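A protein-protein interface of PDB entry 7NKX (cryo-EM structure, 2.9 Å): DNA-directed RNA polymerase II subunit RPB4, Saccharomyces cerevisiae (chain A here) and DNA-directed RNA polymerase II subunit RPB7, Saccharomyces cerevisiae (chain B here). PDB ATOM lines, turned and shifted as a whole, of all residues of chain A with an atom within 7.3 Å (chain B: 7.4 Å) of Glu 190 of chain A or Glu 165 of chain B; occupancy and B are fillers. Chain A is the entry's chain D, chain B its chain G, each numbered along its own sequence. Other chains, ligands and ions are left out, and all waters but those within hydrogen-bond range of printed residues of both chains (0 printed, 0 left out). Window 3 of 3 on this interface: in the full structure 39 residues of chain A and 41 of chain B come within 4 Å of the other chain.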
ATOM      1  N   ALA A 184      -5.544  -6.803   5.229  1.00  0.00           N
ATOM      2  CA  ALA A 184      -5.649  -5.374   5.479  1.00  0.00           C
ATOM      3  C   ALA A 184      -4.359  -4.688   5.054  1.00  0.00           C
ATOM      4  O   ALA A 184      -3.263  -5.166   5.367  1.00  0.00           O
ATOM      5  CB  ALA A 184      -5.933  -5.097   6.955  1.00  0.00           C
ATOM      6  N   CYS A 185      -4.497  -3.577   4.334  1.00  0.00           N
ATOM      7  CA  CYS A 185      -3.371  -2.772   3.892  1.00  0.00           C
ATOM      8  C   CYS A 185      -3.689  -1.307   4.132  1.00  0.00           C
ATOM      9  O   CYS A 185      -4.855  -0.905   4.161  1.00  0.00           O
ATOM     10  CB  CYS A 185      -3.057  -2.997   2.409  1.00  0.00           C
ATOM     11  SG  CYS A 185      -2.219  -4.539   2.042  1.00  0.00           S
ATOM     12  N   ASP A 186      -2.631  -0.514   4.309  1.00  0.00           N
ATOM     13  CA  ASP A 186      -2.750   0.918   4.548  1.00  0.00           C
ATOM     14  C   ASP A 186      -1.843   1.775   3.681  1.00  0.00           C
ATOM     15  O   ASP A 186      -2.152   2.960   3.497  1.00  0.00           O
ATOM     16  CB  ASP A 186      -2.472   1.234   6.029  1.00  0.00           C
ATOM     17  CG  ASP A 186      -1.151   0.658   6.522  1.00  0.00           C
ATOM     18  OD1 ASP A 186      -1.151   0.030   7.601  1.00  0.00           O
ATOM     19  OD2 ASP A 186      -0.115   0.833   5.846  1.00  0.00           O
ATOM     20  N   THR A 187      -0.749   1.234   3.142  1.00  0.00           N
ATOM     21  CA  THR A 187       0.209   2.004   2.363  1.00  0.00           C
ATOM     22  C   THR A 187       0.690   1.208   1.158  1.00  0.00           C
ATOM     23  O   THR A 187       0.723  -0.029   1.171  1.00  0.00           O
ATOM     24  CB  THR A 187       1.414   2.428   3.214  1.00  0.00           C
ATOM     25  OG1 THR A 187       1.957   1.285   3.886  1.00  0.00           O
ATOM     26  CG2 THR A 187       1.011   3.483   4.235  1.00  0.00           C
ATOM     27  N   ALA A 188       1.076   1.952   0.117  1.00  0.00           N
ATOM     28  CA  ALA A 188       1.499   1.336  -1.136  1.00  0.00           C
ATOM     29  C   ALA A 188       2.745   0.487  -0.943  1.00  0.00           C
ATOM     30  O   ALA A 188       2.828  -0.629  -1.464  1.00  0.00           O
ATOM     31  CB  ALA A 188       1.762   2.412  -2.188  1.00  0.00           C
ATOM     32  N   ASP A 189       3.733   1.006  -0.211  1.00  0.00           N
ATOM     33  CA  ASP A 189       4.964   0.257   0.008  1.00  0.00           C
ATOM     34  C   ASP A 189       4.689  -1.037   0.759  1.00  0.00           C
ATOM     35  O   ASP A 189       5.239  -2.095   0.420  1.00  0.00           O
ATOM     36  CB  ASP A 189       5.968   1.118   0.775  1.00  0.00           C
ATOM     37  CG  ASP A 189       7.298   0.425   0.975  1.00  0.00           C
ATOM     38  OD1 ASP A 189       7.657  -0.429   0.138  1.00  0.00           O
ATOM     39  OD2 ASP A 189       7.985   0.734   1.971  1.00  0.00           O
ATOM     40  N   GLU A 190       3.831  -0.972   1.781  1.00  0.00           N
ATOM     41  CA  GLU A 190       3.486  -2.174   2.525  1.00  0.00           C
ATOM     42  C   GLU A 190       2.778  -3.181   1.630  1.00  0.00           C
ATOM     43  O   GLU A 190       3.047  -4.383   1.708  1.00  0.00           O
ATOM     44  CB  GLU A 190       2.620  -1.821   3.740  1.00  0.00           C
ATOM     45  CG  GLU A 190       2.574  -2.848   4.905  1.00  0.00           C
ATOM     46  CD  GLU A 190       3.926  -3.415   5.353  1.00  0.00           C
ATOM     47  OE1 GLU A 190       4.979  -2.806   5.076  1.00  0.00           O
ATOM     48  OE2 GLU A 190       3.928  -4.490   5.987  1.00  0.00           O
ATOM     49  N   ALA A 191       1.882  -2.711   0.755  1.00  0.00           N
ATOM     50  CA  ALA A 191       1.210  -3.630  -0.163  1.00  0.00           C
ATOM     51  C   ALA A 191       2.198  -4.280  -1.128  1.00  0.00           C
ATOM     52  O   ALA A 191       2.122  -5.489  -1.391  1.00  0.00           O
ATOM     53  CB  ALA A 191       0.120  -2.890  -0.939  1.00  0.00           C
ATOM     54  N   LYS A 192       3.127  -3.493  -1.673  1.00  0.00           N
ATOM     55  CA  LYS A 192       4.068  -4.038  -2.645  1.00  0.00           C
ATOM     56  C   LYS A 192       4.999  -5.061  -2.004  1.00  0.00           C
ATOM     57  O   LYS A 192       5.306  -6.092  -2.615  1.00  0.00           O
ATOM     58  CB  LYS A 192       4.871  -2.909  -3.303  1.00  0.00           C
ATOM     59  CG  LYS A 192       4.068  -1.929  -4.185  1.00  0.00           C
ATOM     60  CD  LYS A 192       3.306  -2.569  -5.350  1.00  0.00           C
ATOM     61  CE  LYS A 192       1.856  -2.102  -5.403  1.00  0.00           C
ATOM     62  NZ  LYS A 192       1.219  -2.372  -6.721  1.00  0.00           N
ATOM     63  N   THR A 193       5.466  -4.802  -0.777  1.00  0.00           N
ATOM     64  CA  THR A 193       6.299  -5.807  -0.113  1.00  0.00           C
ATOM     65  C   THR A 193       5.460  -6.998   0.345  1.00  0.00           C
ATOM     66  O   THR A 193       5.982  -8.109   0.496  1.00  0.00           O
ATOM     67  CB  THR A 193       7.074  -5.210   1.069  1.00  0.00           C
ATOM     68  OG1 THR A 193       7.899  -6.226   1.651  1.00  0.00           O
ATOM     69  CG2 THR A 193       6.152  -4.697   2.149  1.00  0.00           C
ATOM     70  N   LEU A 194       4.159  -6.784   0.579  1.00  0.00           N
ATOM     71  CA  LEU A 194       3.243  -7.903   0.779  1.00  0.00           C
ATOM     72  C   LEU A 194       3.254  -8.850  -0.406  1.00  0.00           C
ATOM     73  O   LEU A 194       3.458 -10.060  -0.250  1.00  0.00           O
ATOM     74  CB  LEU A 194       1.817  -7.384   0.994  1.00  0.00           C
ATOM     75  CG  LEU A 194       0.827  -8.153   1.865  1.00  0.00           C
ATOM     76  CD1 LEU A 194       1.361  -8.456   3.225  1.00  0.00           C
ATOM     77  CD2 LEU A 194      -0.466  -7.370   1.972  1.00  0.00           C
ATOM     78  N   ILE A 195       3.035  -8.309  -1.598  1.00  0.00           N
ATOM     79  CA  ILE A 195       2.818  -9.095  -2.809  1.00  0.00           C
ATOM     80  C   ILE A 195       3.799  -8.594  -3.872  1.00  0.00           C
ATOM     81  O   ILE A 195       3.461  -7.735  -4.696  1.00  0.00           O
ATOM     82  CB  ILE A 195       1.315  -9.087  -3.173  1.00  0.00           C
ATOM     83  CG1 ILE A 195       0.780  -7.704  -3.593  1.00  0.00           C
ATOM     84  CG2 ILE A 195       0.504  -9.654  -2.003  1.00  0.00           C
ATOM     85  CD1 ILE A 195      -0.717  -7.653  -3.847  1.00  0.00           C
ATOM     86  N   VAL B  86       1.522 -14.120   3.370  1.00  0.00           N
ATOM     87  CA  VAL B  86       1.484 -13.890   4.811  1.00  0.00           C
ATOM     88  C   VAL B  86       0.042 -14.014   5.267  1.00  0.00           C
ATOM     89  O   VAL B  86      -0.878 -13.456   4.658  1.00  0.00           O
ATOM     90  CB  VAL B  86       2.078 -12.525   5.206  1.00  0.00           C
ATOM     91  CG1 VAL B  86       1.150 -11.375   4.872  1.00  0.00           C
ATOM     92  CG2 VAL B  86       2.351 -12.492   6.697  1.00  0.00           C
ATOM     93  N   ARG B 144       0.595 -12.683  13.082  1.00  0.00           N
ATOM     94  CA  ARG B 144       0.766 -12.708  11.632  1.00  0.00           C
ATOM     95  C   ARG B 144       2.121 -13.310  11.244  1.00  0.00           C
ATOM     96  O   ARG B 144       3.167 -12.793  11.653  1.00  0.00           O
ATOM     97  CB  ARG B 144       0.586 -11.269  11.154  1.00  0.00           C
ATOM     98  CG  ARG B 144       0.766 -10.927   9.700  1.00  0.00           C
ATOM     99  CD  ARG B 144      -0.121  -9.704   9.414  1.00  0.00           C
ATOM    100  NE  ARG B 144      -0.072  -9.219   8.042  1.00  0.00           N
ATOM    101  CZ  ARG B 144       0.977  -8.614   7.491  1.00  0.00           C
ATOM    102  NH1 ARG B 144       2.093  -8.394   8.173  1.00  0.00           N
ATOM    103  NH2 ARG B 144       0.898  -8.202   6.241  1.00  0.00           N
ATOM    104  N   LYS B 146       4.513 -15.374   7.919  1.00  0.00           N
ATOM    105  CA  LYS B 146       4.674 -15.592   6.479  1.00  0.00           C
ATOM    106  C   LYS B 146       5.075 -17.041   6.256  1.00  0.00           C
ATOM    107  O   LYS B 146       6.064 -17.502   6.824  1.00  0.00           O
ATOM    108  CB  LYS B 146       5.734 -14.704   5.811  1.00  0.00           C
ATOM    109  CG  LYS B 146       5.766 -13.220   6.104  1.00  0.00           C
ATOM    110  CD  LYS B 146       6.938 -12.585   5.354  1.00  0.00           C
ATOM    111  CE  LYS B 146       6.678 -11.129   4.996  1.00  0.00           C
ATOM    112  NZ  LYS B 146       7.715 -10.590   4.075  1.00  0.00           N
ATOM    113  N   SER B 162       7.858 -17.559   9.233  1.00  0.00           N
ATOM    114  CA  SER B 162       8.859 -16.661   9.785  1.00  0.00           C
ATOM    115  C   SER B 162       8.199 -15.332  10.114  1.00  0.00           C
ATOM    116  O   SER B 162       7.096 -15.033   9.649  1.00  0.00           O
ATOM    117  CB  SER B 162      10.006 -16.434   8.795  1.00  0.00           C
ATOM    118  OG  SER B 162       9.543 -15.759   7.637  1.00  0.00           O
ATOM    119  N   ILE B 163       8.894 -14.531  10.920  1.00  0.00           N
ATOM    120  CA  ILE B 163       8.424 -13.205  11.325  1.00  0.00           C
ATOM    121  C   ILE B 163       9.650 -12.289  11.341  1.00  0.00           C
ATOM    122  O   ILE B 163      10.480 -12.342  12.255  1.00  0.00           O
ATOM    123  CB  ILE B 163       7.638 -13.215  12.655  1.00  0.00           C
ATOM    124  CG1 ILE B 163       8.485 -13.430  13.928  1.00  0.00           C
ATOM    125  CG2 ILE B 163       6.493 -14.226  12.605  1.00  0.00           C
ATOM    126  CD1 ILE B 163       7.695 -13.475  15.227  1.00  0.00           C
ATOM    127  N   LYS B 164       9.873 -11.568  10.238  1.00  0.00           N
ATOM    128  CA  LYS B 164      11.018 -10.657  10.185  1.00  0.00           C
ATOM    129  C   LYS B 164      10.680  -9.303   9.586  1.00  0.00           C
ATOM    130  O   LYS B 164      11.092  -8.274  10.130  1.00  0.00           O
ATOM    131  CB  LYS B 164      12.180 -11.350   9.397  1.00  0.00           C
ATOM    132  CG  LYS B 164      11.857 -11.882   7.978  1.00  0.00           C
ATOM    133  CD  LYS B 164      12.154 -10.918   6.824  1.00  0.00           C
ATOM    134  CE  LYS B 164      11.758 -11.545   5.494  1.00  0.00           C
ATOM    135  NZ  LYS B 164      12.166 -10.723   4.325  1.00  0.00           N
ATOM    136  N   GLU B 165       9.946  -9.281   8.482  1.00  0.00           N
ATOM    137  CA  GLU B 165       9.597  -8.050   7.793  1.00  0.00           C
ATOM    138  C   GLU B 165       8.711  -7.176   8.709  1.00  0.00           C
ATOM    139  O   GLU B 165       8.189  -7.623   9.734  1.00  0.00           O
ATOM    140  CB  GLU B 165       9.129  -8.470   6.373  1.00  0.00           C
ATOM    141  CG  GLU B 165       8.689  -7.477   5.272  1.00  0.00           C
ATOM    142  CD  GLU B 165       7.514  -6.652   5.606  1.00  0.00           C
ATOM    143  OE1 GLU B 165       6.787  -7.124   6.477  1.00  0.00           O
ATOM    144  OE2 GLU B 165       7.318  -5.566   5.023  1.00  0.00           O
ATOM    145  N   ASP B 166       8.555  -5.916   8.314  1.00  0.00           N
ATOM    146  CA  ASP B 166       7.771  -4.899   9.023  1.00  0.00           C
ATOM    147  C   ASP B 166       6.285  -5.240   9.149  1.00  0.00           C
ATOM    148  O   ASP B 166       5.704  -5.906   8.298  1.00  0.00           O
ATOM    149  CB  ASP B 166       7.908  -3.545   8.322  1.00  0.00           C
ATOM    150  CG  ASP B 166       9.352  -3.129   8.121  1.00  0.00           C
ATOM    151  OD1 ASP B 166       9.640  -2.448   7.114  1.00  0.00           O
ATOM    152  OD2 ASP B 166      10.197  -3.481   8.968  1.00  0.00           O
ATOM    153  N   TYR B 167       5.672  -4.826  10.262  1.00  0.00           N
ATOM    154  CA  TYR B 167       4.234  -5.026  10.542  1.00  0.00           C
ATOM    155  C   TYR B 167       3.891  -6.490  10.841  1.00  0.00           C
ATOM    156  O   TYR B 167       2.705  -6.826  10.933  1.00  0.00           O
ATOM    157  CB  TYR B 167       3.396  -4.425   9.383  1.00  0.00           C
ATOM    158  CG  TYR B 167       1.883  -4.596   9.338  1.00  0.00           C
ATOM    159  CD1 TYR B 167       1.092  -4.484  10.477  1.00  0.00           C
ATOM    160  CD2 TYR B 167       1.253  -4.889   8.135  1.00  0.00           C
ATOM    161  CE1 TYR B 167      -0.281  -4.649  10.412  1.00  0.00           C
ATOM    162  CE2 TYR B 167      -0.115  -5.055   8.061  1.00  0.00           C
ATOM    163  CZ  TYR B 167      -0.879  -4.935   9.201  1.00  0.00           C
ATOM    164  OH  TYR B 167      -2.244  -5.103   9.125  1.00  0.00           O
ATOM    165  N   LEU B 168       4.866  -7.376  11.075  1.00  0.00           N
ATOM    166  CA  LEU B 168       4.505  -8.749  11.400  1.00  0.00           C
ATOM    167  C   LEU B 168       4.676  -8.996  12.891  1.00  0.00           C
ATOM    168  O   LEU B 168       5.397  -8.284  13.596  1.00  0.00           O
ATOM    169  CB  LEU B 168       5.430  -9.757  10.711  1.00  0.00           C
ATOM    170  CG  LEU B 168       5.638  -9.878   9.202  1.00  0.00           C
ATOM    171  CD1 LEU B 168       7.014 -10.460   8.914  1.00  0.00           C
ATOM    172  CD2 LEU B 168       4.597 -10.756   8.572  1.00  0.00           C
ATOM    173  N   GLY B 169       3.985 -10.035  13.350  1.00  0.00           N
ATOM    174  CA  GLY B 169       3.996 -10.490  14.724  1.00  0.00           C
ATOM    175  C   GLY B 169       2.697 -10.048  15.362  1.00  0.00           C
ATOM    176  O   GLY B 169       1.700  -9.881  14.654  1.00  0.00           O
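OE2 of Glu 165 of chain B lies close to OG1 of Thr 193 of chain A (3.5 Å).
OE2 of Glu 190 of chain A lies close to O of Asp 166 of chain B (3.2 Å).
The backbone carbonyl oxygen (O) of Tyr 167 of chain B lies within hydrogen-bond range of the guanidinium group (NH1) of Arg 144 of chain B (3.2 Å).
O of Arg 144 of chain B sits at hydrogen-bond distance from N of Gly 169 of chain B, 3.3 Å away.
Among the printed residues, merely in contact across the chains: Leu 194 of chain A with Arg 144 of chain B (3.1 Å), Leu 194 of chain A with Val 86 of chain B (3.4 Å), Glu 190 of chain A with Tyr 167 of chain B (3.4 Å), Glu 190 of chain A with Glu 165 of chain B (3.6 Å) and Ala 184 of chain A with Tyr 167 of chain B (3.9 Å).
Of chain B, only Glu 165, Asp 166 and Tyr 167 come within 4 Å of Glu 190 of chain A.
Of chain A, only Glu 190 (3.6 Å) and Thr 193 (3.2 Å) come within 4 Å of Glu 165 of chain B.
Of the printed residues of chain A, Arg 144 of chain B touches Leu 194 (3.1 Å).
Printed residues of chain B within 4 Å of Leu 194 of chain A: Val 86 and Arg 144.
The nearest residue of chain B that does not touch Glu 190 of chain A is Arg 144 of chain B (4.8 Å).
The nearest residue of chain A that does not touch Glu 165 of chain B is Leu 194 of chain A (5.6 Å).
Printed residues of chain B that touch a printed residue of chain A: Val 86, Arg 144, Glu 165, Asp 166 and Tyr 167.
Hydrophobic or aromatic side chains of chain B within 4 Å of the printed part of chain A: Val 86 and Tyr 167.
Along chain B the printed residues that touch a printed residue of chain A span positions 86 to 167.
Hydrophobic or aromatic side chains of chain A within 4 Å of the printed part of chain B: Leu 194.
Among the printed residues, 7 pairs touch across the chains.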
